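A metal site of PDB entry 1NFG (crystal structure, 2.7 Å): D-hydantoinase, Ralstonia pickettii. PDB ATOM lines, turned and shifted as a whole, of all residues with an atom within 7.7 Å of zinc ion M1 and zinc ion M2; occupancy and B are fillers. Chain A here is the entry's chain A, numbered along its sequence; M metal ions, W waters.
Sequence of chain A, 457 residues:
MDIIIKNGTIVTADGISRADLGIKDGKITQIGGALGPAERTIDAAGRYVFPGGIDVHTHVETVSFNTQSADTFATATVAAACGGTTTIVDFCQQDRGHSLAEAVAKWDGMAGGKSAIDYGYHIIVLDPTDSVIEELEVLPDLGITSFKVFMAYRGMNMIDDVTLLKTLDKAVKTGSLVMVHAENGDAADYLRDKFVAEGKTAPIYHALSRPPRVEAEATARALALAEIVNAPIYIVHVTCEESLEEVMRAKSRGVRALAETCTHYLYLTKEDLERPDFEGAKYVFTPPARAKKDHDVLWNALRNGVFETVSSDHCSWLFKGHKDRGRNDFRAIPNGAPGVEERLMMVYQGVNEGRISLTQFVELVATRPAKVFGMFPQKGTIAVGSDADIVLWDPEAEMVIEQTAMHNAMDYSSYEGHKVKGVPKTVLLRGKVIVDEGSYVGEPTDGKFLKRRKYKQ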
ATOM      1  N   HIS A  57     -14.886  14.544  -5.048  1.00  0.00           N
ATOM      2  CA  HIS A  57     -14.776  13.144  -5.446  1.00  0.00           C
ATOM      3  C   HIS A  57     -16.088  12.389  -5.266  1.00  0.00           C
ATOM      4  O   HIS A  57     -16.276  11.694  -4.272  1.00  0.00           O
ATOM      5  CB  HIS A  57     -13.667  12.453  -4.650  1.00  0.00           C
ATOM      6  CG  HIS A  57     -13.285  11.109  -5.172  1.00  0.00           C
ATOM      7  ND1 HIS A  57     -12.031  10.570  -5.005  1.00  0.00           N
ATOM      8  CD2 HIS A  57     -13.991  10.174  -5.866  1.00  0.00           C
ATOM      9  CE1 HIS A  57     -11.980   9.374  -5.570  1.00  0.00           C
ATOM     10  NE2 HIS A  57     -13.150   9.114  -6.094  1.00  0.00           N
ATOM     11  N   THR A  58     -16.989  12.540  -6.234  1.00  0.00           N
ATOM     12  CA  THR A  58     -18.281  11.866  -6.194  1.00  0.00           C
ATOM     13  C   THR A  58     -18.616  11.115  -7.477  1.00  0.00           C
ATOM     14  O   THR A  58     -18.120  11.442  -8.562  1.00  0.00           O
ATOM     15  CB  THR A  58     -19.449  12.850  -5.937  1.00  0.00           C
ATOM     16  OG1 THR A  58     -19.460  13.863  -6.956  1.00  0.00           O
ATOM     17  CG2 THR A  58     -19.311  13.499  -4.584  1.00  0.00           C
ATOM     18  N   HIS A  59     -19.460  10.100  -7.323  1.00  0.00           N
ATOM     19  CA  HIS A  59     -19.954   9.290  -8.429  1.00  0.00           C
ATOM     20  C   HIS A  59     -21.448   9.244  -8.163  1.00  0.00           C
ATOM     21  O   HIS A  59     -22.032   8.176  -7.925  1.00  0.00           O
ATOM     22  CB  HIS A  59     -19.340   7.897  -8.376  1.00  0.00           C
ATOM     23  CG  HIS A  59     -17.839   7.889  -8.478  1.00  0.00           C
ATOM     24  ND1 HIS A  59     -17.167   8.408  -9.566  1.00  0.00           N
ATOM     25  CD2 HIS A  59     -16.891   7.447  -7.623  1.00  0.00           C
ATOM     26  CE1 HIS A  59     -15.874   8.277  -9.378  1.00  0.00           C
ATOM     27  NE2 HIS A  59     -15.675   7.701  -8.211  1.00  0.00           N
ATOM     28  N   PHE A  91     -17.481  12.770 -11.314  1.00  0.00           N
ATOM     29  CA  PHE A  91     -16.631  12.191 -12.342  1.00  0.00           C
ATOM     30  C   PHE A  91     -17.457  11.832 -13.560  1.00  0.00           C
ATOM     31  O   PHE A  91     -18.183  10.830 -13.566  1.00  0.00           O
ATOM     32  CB  PHE A  91     -15.912  10.946 -11.794  1.00  0.00           C
ATOM     33  CG  PHE A  91     -14.688  11.262 -10.985  1.00  0.00           C
ATOM     34  CD1 PHE A  91     -13.521  11.675 -11.617  1.00  0.00           C
ATOM     35  CD2 PHE A  91     -14.711  11.204  -9.594  1.00  0.00           C
ATOM     36  CE1 PHE A  91     -12.391  12.030 -10.874  1.00  0.00           C
ATOM     37  CE2 PHE A  91     -13.592  11.546  -8.840  1.00  0.00           C
ATOM     38  CZ  PHE A  91     -12.423  11.962  -9.486  1.00  0.00           C
ATOM     39  N   ILE A 124     -13.315  11.438 -17.014  1.00  0.00           N
ATOM     40  CA  ILE A 124     -12.638  10.158 -16.969  1.00  0.00           C
ATOM     41  C   ILE A 124     -12.347   9.698 -18.391  1.00  0.00           C
ATOM     42  O   ILE A 124     -13.251   9.611 -19.219  1.00  0.00           O
ATOM     43  CB  ILE A 124     -13.486   9.057 -16.333  1.00  0.00           C
ATOM     44  CG1 ILE A 124     -13.670   9.315 -14.841  1.00  0.00           C
ATOM     45  CG2 ILE A 124     -12.813   7.711 -16.533  1.00  0.00           C
ATOM     46  CD1 ILE A 124     -14.368   8.203 -14.107  1.00  0.00           C
ATOM     47  N   KCX A 148      -9.120  12.377 -15.398  1.00  0.00           N
ATOM     48  CA  KCX A 148      -8.954  11.237 -14.522  1.00  0.00           C
ATOM     49  CB  KCX A 148     -10.151  11.170 -13.569  1.00  0.00           C
ATOM     50  CG  KCX A 148     -10.428   9.786 -13.085  1.00  0.00           C
ATOM     51  CD  KCX A 148      -9.559   9.416 -11.911  1.00  0.00           C
ATOM     52  CE  KCX A 148     -10.502   9.293 -10.773  1.00  0.00           C
ATOM     53  NZ  KCX A 148     -10.325   8.091 -10.031  1.00  0.00           N
ATOM     54  C   KCX A 148      -8.790   9.903 -15.264  1.00  0.00           C
ATOM     55  O   KCX A 148      -9.568   9.591 -16.178  1.00  0.00           O
ATOM     56  CX  KCX A 148     -11.232   7.528  -9.226  1.00  0.00           C
ATOM     57  OQ1 KCX A 148     -10.871   6.468  -8.649  1.00  0.00           O
ATOM     58  OQ2 KCX A 148     -12.401   8.064  -9.074  1.00  0.00           O
ATOM     59  N   VAL A 149      -7.784   9.116 -14.865  1.00  0.00           N
ATOM     60  CA  VAL A 149      -7.524   7.809 -15.463  1.00  0.00           C
ATOM     61  C   VAL A 149      -7.377   6.730 -14.388  1.00  0.00           C
ATOM     62  O   VAL A 149      -7.107   7.027 -13.225  1.00  0.00           O
ATOM     63  CB  VAL A 149      -6.249   7.819 -16.334  1.00  0.00           C
ATOM     64  CG1 VAL A 149      -6.475   8.696 -17.559  1.00  0.00           C
ATOM     65  CG2 VAL A 149      -5.062   8.332 -15.532  1.00  0.00           C
ATOM     66  N   PHE A 150      -7.574   5.470 -14.777  1.00  0.00           N
ATOM     67  CA  PHE A 150      -7.478   4.353 -13.852  1.00  0.00           C
ATOM     68  C   PHE A 150      -6.320   3.410 -14.181  1.00  0.00           C
ATOM     69  O   PHE A 150      -6.067   3.103 -15.351  1.00  0.00           O
ATOM     70  CB  PHE A 150      -8.782   3.551 -13.846  1.00  0.00           C
ATOM     71  CG  PHE A 150      -9.925   4.269 -13.199  1.00  0.00           C
ATOM     72  CD1 PHE A 150     -10.504   5.377 -13.807  1.00  0.00           C
ATOM     73  CD2 PHE A 150     -10.410   3.847 -11.959  1.00  0.00           C
ATOM     74  CE1 PHE A 150     -11.562   6.070 -13.179  1.00  0.00           C
ATOM     75  CE2 PHE A 150     -11.461   4.533 -11.332  1.00  0.00           C
ATOM     76  CZ  PHE A 150     -12.034   5.648 -11.945  1.00  0.00           C
ATOM     77  N   TYR A 153      -8.737  -2.141 -12.697  1.00  0.00           N
ATOM     78  CA  TYR A 153     -10.006  -2.481 -13.340  1.00  0.00           C
ATOM     79  C   TYR A 153      -9.806  -2.871 -14.807  1.00  0.00           C
ATOM     80  O   TYR A 153     -10.177  -2.127 -15.709  1.00  0.00           O
ATOM     81  CB  TYR A 153     -10.985  -1.319 -13.255  1.00  0.00           C
ATOM     82  CG  TYR A 153     -11.305  -0.889 -11.841  1.00  0.00           C
ATOM     83  CD1 TYR A 153     -11.628  -1.829 -10.866  1.00  0.00           C
ATOM     84  CD2 TYR A 153     -11.328   0.463 -11.489  1.00  0.00           C
ATOM     85  CE1 TYR A 153     -11.974  -1.430  -9.569  1.00  0.00           C
ATOM     86  CE2 TYR A 153     -11.670   0.868 -10.198  1.00  0.00           C
ATOM     87  CZ  TYR A 153     -11.988  -0.080  -9.245  1.00  0.00           C
ATOM     88  OH  TYR A 153     -12.345   0.325  -7.970  1.00  0.00           O
ATOM     89  N   VAL A 180      -5.525  10.312 -10.687  1.00  0.00           N
ATOM     90  CA  VAL A 180      -5.354   8.903 -10.944  1.00  0.00           C
ATOM     91  C   VAL A 180      -5.704   7.959  -9.798  1.00  0.00           C
ATOM     92  O   VAL A 180      -5.397   8.222  -8.639  1.00  0.00           O
ATOM     93  CB  VAL A 180      -3.898   8.592 -11.409  1.00  0.00           C
ATOM     94  CG1 VAL A 180      -2.915   9.161 -10.432  1.00  0.00           C
ATOM     95  CG2 VAL A 180      -3.697   7.097 -11.536  1.00  0.00           C
ATOM     96  N   HIS A 181      -6.369   6.869 -10.158  1.00  0.00           N
ATOM     97  CA  HIS A 181      -6.740   5.807  -9.225  1.00  0.00           C
ATOM     98  C   HIS A 181      -5.505   4.906  -9.300  1.00  0.00           C
ATOM     99  O   HIS A 181      -5.291   4.229 -10.303  1.00  0.00           O
ATOM    100  CB  HIS A 181      -7.975   5.079  -9.743  1.00  0.00           C
ATOM    101  CG  HIS A 181      -8.309   3.840  -8.981  1.00  0.00           C
ATOM    102  ND1 HIS A 181      -9.419   3.750  -8.169  1.00  0.00           N
ATOM    103  CD2 HIS A 181      -7.701   2.631  -8.920  1.00  0.00           C
ATOM    104  CE1 HIS A 181      -9.480   2.536  -7.639  1.00  0.00           C
ATOM    105  NE2 HIS A 181      -8.449   1.837  -8.082  1.00  0.00           N
ATOM    106  N   ALA A 182      -4.686   4.922  -8.255  1.00  0.00           N
ATOM    107  CA  ALA A 182      -3.445   4.140  -8.276  1.00  0.00           C
ATOM    108  C   ALA A 182      -3.423   2.791  -7.586  1.00  0.00           C
ATOM    109  O   ALA A 182      -3.228   2.677  -6.375  1.00  0.00           O
ATOM    110  CB  ALA A 182      -2.296   5.013  -7.767  1.00  0.00           C
ATOM    111  N   GLU A 183      -3.609   1.749  -8.386  1.00  0.00           N
ATOM    112  CA  GLU A 183      -3.550   0.375  -7.907  1.00  0.00           C
ATOM    113  C   GLU A 183      -3.005  -0.399  -9.081  1.00  0.00           C
ATOM    114  O   GLU A 183      -3.281  -0.055 -10.230  1.00  0.00           O
ATOM    115  CB  GLU A 183      -4.926  -0.170  -7.581  1.00  0.00           C
ATOM    116  CG  GLU A 183      -5.355   0.024  -6.166  1.00  0.00           C
ATOM    117  CD  GLU A 183      -6.695  -0.619  -5.936  1.00  0.00           C
ATOM    118  OE1 GLU A 183      -7.581  -0.363  -6.766  1.00  0.00           O
ATOM    119  OE2 GLU A 183      -6.870  -1.371  -4.961  1.00  0.00           O
ATOM    120  N   VAL A 236      -5.875  10.302  -6.071  1.00  0.00           N
ATOM    121  CA  VAL A 236      -7.128  10.186  -5.356  1.00  0.00           C
ATOM    122  C   VAL A 236      -7.037   9.080  -4.313  1.00  0.00           C
ATOM    123  O   VAL A 236      -6.226   8.168  -4.435  1.00  0.00           O
ATOM    124  CB  VAL A 236      -8.323   9.887  -6.318  1.00  0.00           C
ATOM    125  CG1 VAL A 236      -8.402  10.952  -7.398  1.00  0.00           C
ATOM    126  CG2 VAL A 236      -8.190   8.505  -6.928  1.00  0.00           C
ATOM    127  N   HIS A 237      -7.883   9.177  -3.296  1.00  0.00           N
ATOM    128  CA  HIS A 237      -7.932   8.238  -2.194  1.00  0.00           C
ATOM    129  C   HIS A 237      -6.648   7.525  -1.763  1.00  0.00           C
ATOM    130  O   HIS A 237      -6.479   6.334  -2.005  1.00  0.00           O
ATOM    131  CB  HIS A 237      -9.048   7.195  -2.432  1.00  0.00           C
ATOM    132  CG  HIS A 237      -8.978   6.501  -3.762  1.00  0.00           C
ATOM    133  ND1 HIS A 237      -7.803   6.043  -4.310  1.00  0.00           N
ATOM    134  CD2 HIS A 237      -9.952   6.166  -4.640  1.00  0.00           C
ATOM    135  CE1 HIS A 237      -8.054   5.456  -5.465  1.00  0.00           C
ATOM    136  NE2 HIS A 237      -9.349   5.529  -5.687  1.00  0.00           N
ATOM    137  N   GLU A 260      -5.117  13.148  -1.696  1.00  0.00           N
ATOM    138  CA  GLU A 260      -6.286  13.343  -0.846  1.00  0.00           C
ATOM    139  C   GLU A 260      -6.600  12.015  -0.151  1.00  0.00           C
ATOM    140  O   GLU A 260      -5.933  11.007  -0.399  1.00  0.00           O
ATOM    141  CB  GLU A 260      -7.498  13.736  -1.690  1.00  0.00           C
ATOM    142  CG  GLU A 260      -7.768  12.762  -2.861  1.00  0.00           C
ATOM    143  CD  GLU A 260      -9.246  12.655  -3.237  1.00  0.00           C
ATOM    144  OE1 GLU A 260      -9.881  13.705  -3.455  1.00  0.00           O
ATOM    145  OE2 GLU A 260      -9.766  11.514  -3.311  1.00  0.00           O
ATOM    146  N   CYS A 262     -10.214   9.872   1.914  1.00  0.00           N
ATOM    147  CA  CYS A 262     -11.658   9.874   1.954  1.00  0.00           C
ATOM    148  C   CYS A 262     -12.137   9.430   3.321  1.00  0.00           C
ATOM    149  O   CYS A 262     -11.584   8.516   3.930  1.00  0.00           O
ATOM    150  CB  CYS A 262     -12.212   8.988   0.828  1.00  0.00           C
ATOM    151  SG  CYS A 262     -11.621   9.452  -0.844  1.00  0.00           S
ATOM    152  N   TYR A 265     -11.611   6.095   5.036  1.00  0.00           N
ATOM    153  CA  TYR A 265     -10.252   5.648   5.267  1.00  0.00           C
ATOM    154  C   TYR A 265      -9.700   6.158   6.592  1.00  0.00           C
ATOM    155  O   TYR A 265      -8.566   5.865   6.965  1.00  0.00           O
ATOM    156  CB  TYR A 265      -9.351   6.068   4.106  1.00  0.00           C
ATOM    157  CG  TYR A 265      -9.731   5.370   2.823  1.00  0.00           C
ATOM    158  CD1 TYR A 265      -9.691   3.979   2.731  1.00  0.00           C
ATOM    159  CD2 TYR A 265     -10.155   6.095   1.716  1.00  0.00           C
ATOM    160  CE1 TYR A 265     -10.076   3.323   1.565  1.00  0.00           C
ATOM    161  CE2 TYR A 265     -10.541   5.455   0.531  1.00  0.00           C
ATOM    162  CZ  TYR A 265     -10.494   4.067   0.470  1.00  0.00           C
ATOM    163  OH  TYR A 265     -10.871   3.434  -0.698  1.00  0.00           O
ATOM    164  N   THR A 286     -12.943   0.435  -2.981  1.00  0.00           N
ATOM    165  CA  THR A 286     -11.564   0.392  -3.427  1.00  0.00           C
ATOM    166  C   THR A 286     -10.860   1.741  -3.439  1.00  0.00           C
ATOM    167  O   THR A 286     -11.436   2.743  -3.858  1.00  0.00           O
ATOM    168  CB  THR A 286     -11.510  -0.222  -4.844  1.00  0.00           C
ATOM    169  OG1 THR A 286     -12.019  -1.555  -4.804  1.00  0.00           O
ATOM    170  CG2 THR A 286     -10.091  -0.225  -5.386  1.00  0.00           C
ATOM    171  N   PRO A 287      -9.598   1.783  -2.987  1.00  0.00           N
ATOM    172  CA  PRO A 287      -8.842   0.640  -2.465  1.00  0.00           C
ATOM    173  C   PRO A 287      -9.509   0.080  -1.217  1.00  0.00           C
ATOM    174  O   PRO A 287     -10.396   0.712  -0.638  1.00  0.00           O
ATOM    175  CB  PRO A 287      -7.464   1.227  -2.210  1.00  0.00           C
ATOM    176  CG  PRO A 287      -7.326   2.204  -3.325  1.00  0.00           C
ATOM    177  CD  PRO A 287      -8.680   2.895  -3.303  1.00  0.00           C
ATOM    178  N   SER A 312     -15.273  12.168  -0.460  1.00  0.00           N
ATOM    179  CA  SER A 312     -16.044  10.973  -0.097  1.00  0.00           C
ATOM    180  C   SER A 312     -15.990   9.747  -1.022  1.00  0.00           C
ATOM    181  O   SER A 312     -16.114   8.619  -0.545  1.00  0.00           O
ATOM    182  CB  SER A 312     -17.521  11.351   0.097  1.00  0.00           C
ATOM    183  OG  SER A 312     -18.113  11.789  -1.126  1.00  0.00           O
ATOM    184  N   ASP A 313     -15.794   9.953  -2.324  1.00  0.00           N
ATOM    185  CA  ASP A 313     -15.799   8.843  -3.282  1.00  0.00           C
ATOM    186  C   ASP A 313     -17.155   8.145  -3.115  1.00  0.00           C
ATOM    187  O   ASP A 313     -17.247   6.915  -3.019  1.00  0.00           O
ATOM    188  CB  ASP A 313     -14.651   7.853  -2.999  1.00  0.00           C
ATOM    189  CG  ASP A 313     -14.450   6.837  -4.136  1.00  0.00           C
ATOM    190  OD1 ASP A 313     -14.847   7.139  -5.290  1.00  0.00           O
ATOM    191  OD2 ASP A 313     -13.894   5.743  -3.883  1.00  0.00           O
ATOM    192  N   HIS A 314     -18.193   8.969  -3.082  1.00  0.00           N
ATOM    193  CA  HIS A 314     -19.574   8.524  -2.917  1.00  0.00           C
ATOM    194  C   HIS A 314     -20.098   7.640  -4.048  1.00  0.00           C
ATOM    195  O   HIS A 314     -20.067   8.010  -5.230  1.00  0.00           O
ATOM    196  CB  HIS A 314     -20.501   9.751  -2.778  1.00  0.00           C
ATOM    197  CG  HIS A 314     -21.939   9.404  -2.590  1.00  0.00           C
ATOM    198  ND1 HIS A 314     -22.464   9.015  -1.368  1.00  0.00           N
ATOM    199  CD2 HIS A 314     -22.964   9.340  -3.475  1.00  0.00           C
ATOM    200  CE1 HIS A 314     -23.741   8.731  -1.516  1.00  0.00           C
ATOM    201  NE2 HIS A 314     -24.075   8.922  -2.774  1.00  0.00           N
ATOM    202  N   CYS A 315     -20.587   6.467  -3.656  1.00  0.00           N
ATOM    203  CA  CYS A 315     -21.161   5.491  -4.578  1.00  0.00           C
ATOM    204  C   CYS A 315     -22.467   5.006  -3.965  1.00  0.00           C
ATOM    205  O   CYS A 315     -22.698   5.143  -2.770  1.00  0.00           O
ATOM    206  CB  CYS A 315     -20.212   4.312  -4.785  1.00  0.00           C
ATOM    207  SG  CYS A 315     -18.750   4.709  -5.750  1.00  0.00           S
HETATM  208 ZN    ZN M   1     -13.687   7.062  -7.182  1.00  0.00          ZN
HETATM  209 ZN    ZN M   2     -11.272   5.012  -7.365  1.00  0.00          ZN
HETATM  210  O   HOH W   1     -14.211   4.180  -8.769  1.00  0.00           O
HETATM  211  O   HOH W   2     -12.844   4.019  -6.220  1.00  0.00           O
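Within 4 Å of zinc ion M1: His 57, His 59, KCX 148 and Asp 313. The nearest printed residue that does not touch zinc ion M1 is His 237 (4.6 Å).
Three residues have an atom within 4 Å of zinc ion M2: KCX 148, His 181 and His 237.
Zinc ion M1 is bound by the side-chain carboxylate (OD1) of Asp 313 (2.2 Å), a ring nitrogen (NE2) of His 59 (2.3 Å), a ring nitrogen (NE2) of His 57 (2.4 Å) and OQ2 of KCX 148 (2.5 Å). Zinc ion M1 has four donor atoms within binding distance.
Zinc ion M2 is bound by OQ1 of KCX 148 (2.0 Å), water W2 (2.2 Å) and a ring nitrogen (ND1) of His 181 (2.4 Å). Zinc ion M2 has three donor atoms within binding distance. Slightly farther from zinc ion M2 lies a ring nitrogen (NE2) of His 237 (2.6 Å).
The side-chain carboxylate (OE2) of Glu 260 sits at hydrogen-bond distance from a ring nitrogen (ND1) of His 57, at 3.0 Å. ND1 of His 181 lies close to NE2 of His 237. NE2 of His 237 lies close to OQ1 of KCX 148, 3.5 Å away. The side-chain carboxylate of Glu 260 sits at hydrogen-bond distance from the backbone NH of His 237 (3.0 Å). O of His 314 is in hydrogen-bond range of N of His 59 (3.0 Å). The backbone NH (N) of His 181 lies within hydrogen-bond range of the backbone carbonyl oxygen (O) of Val 149 (3.2 Å). The side-chain carboxylate (OE1) of Glu 183 is in hydrogen-bond range of a ring nitrogen (NE2) of His 181.
Water W2 bridges the backbone carbonyl oxygen of Thr 286 (3.0 Å) and the side-chain carboxylate of Asp 313 (3.1 Å).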
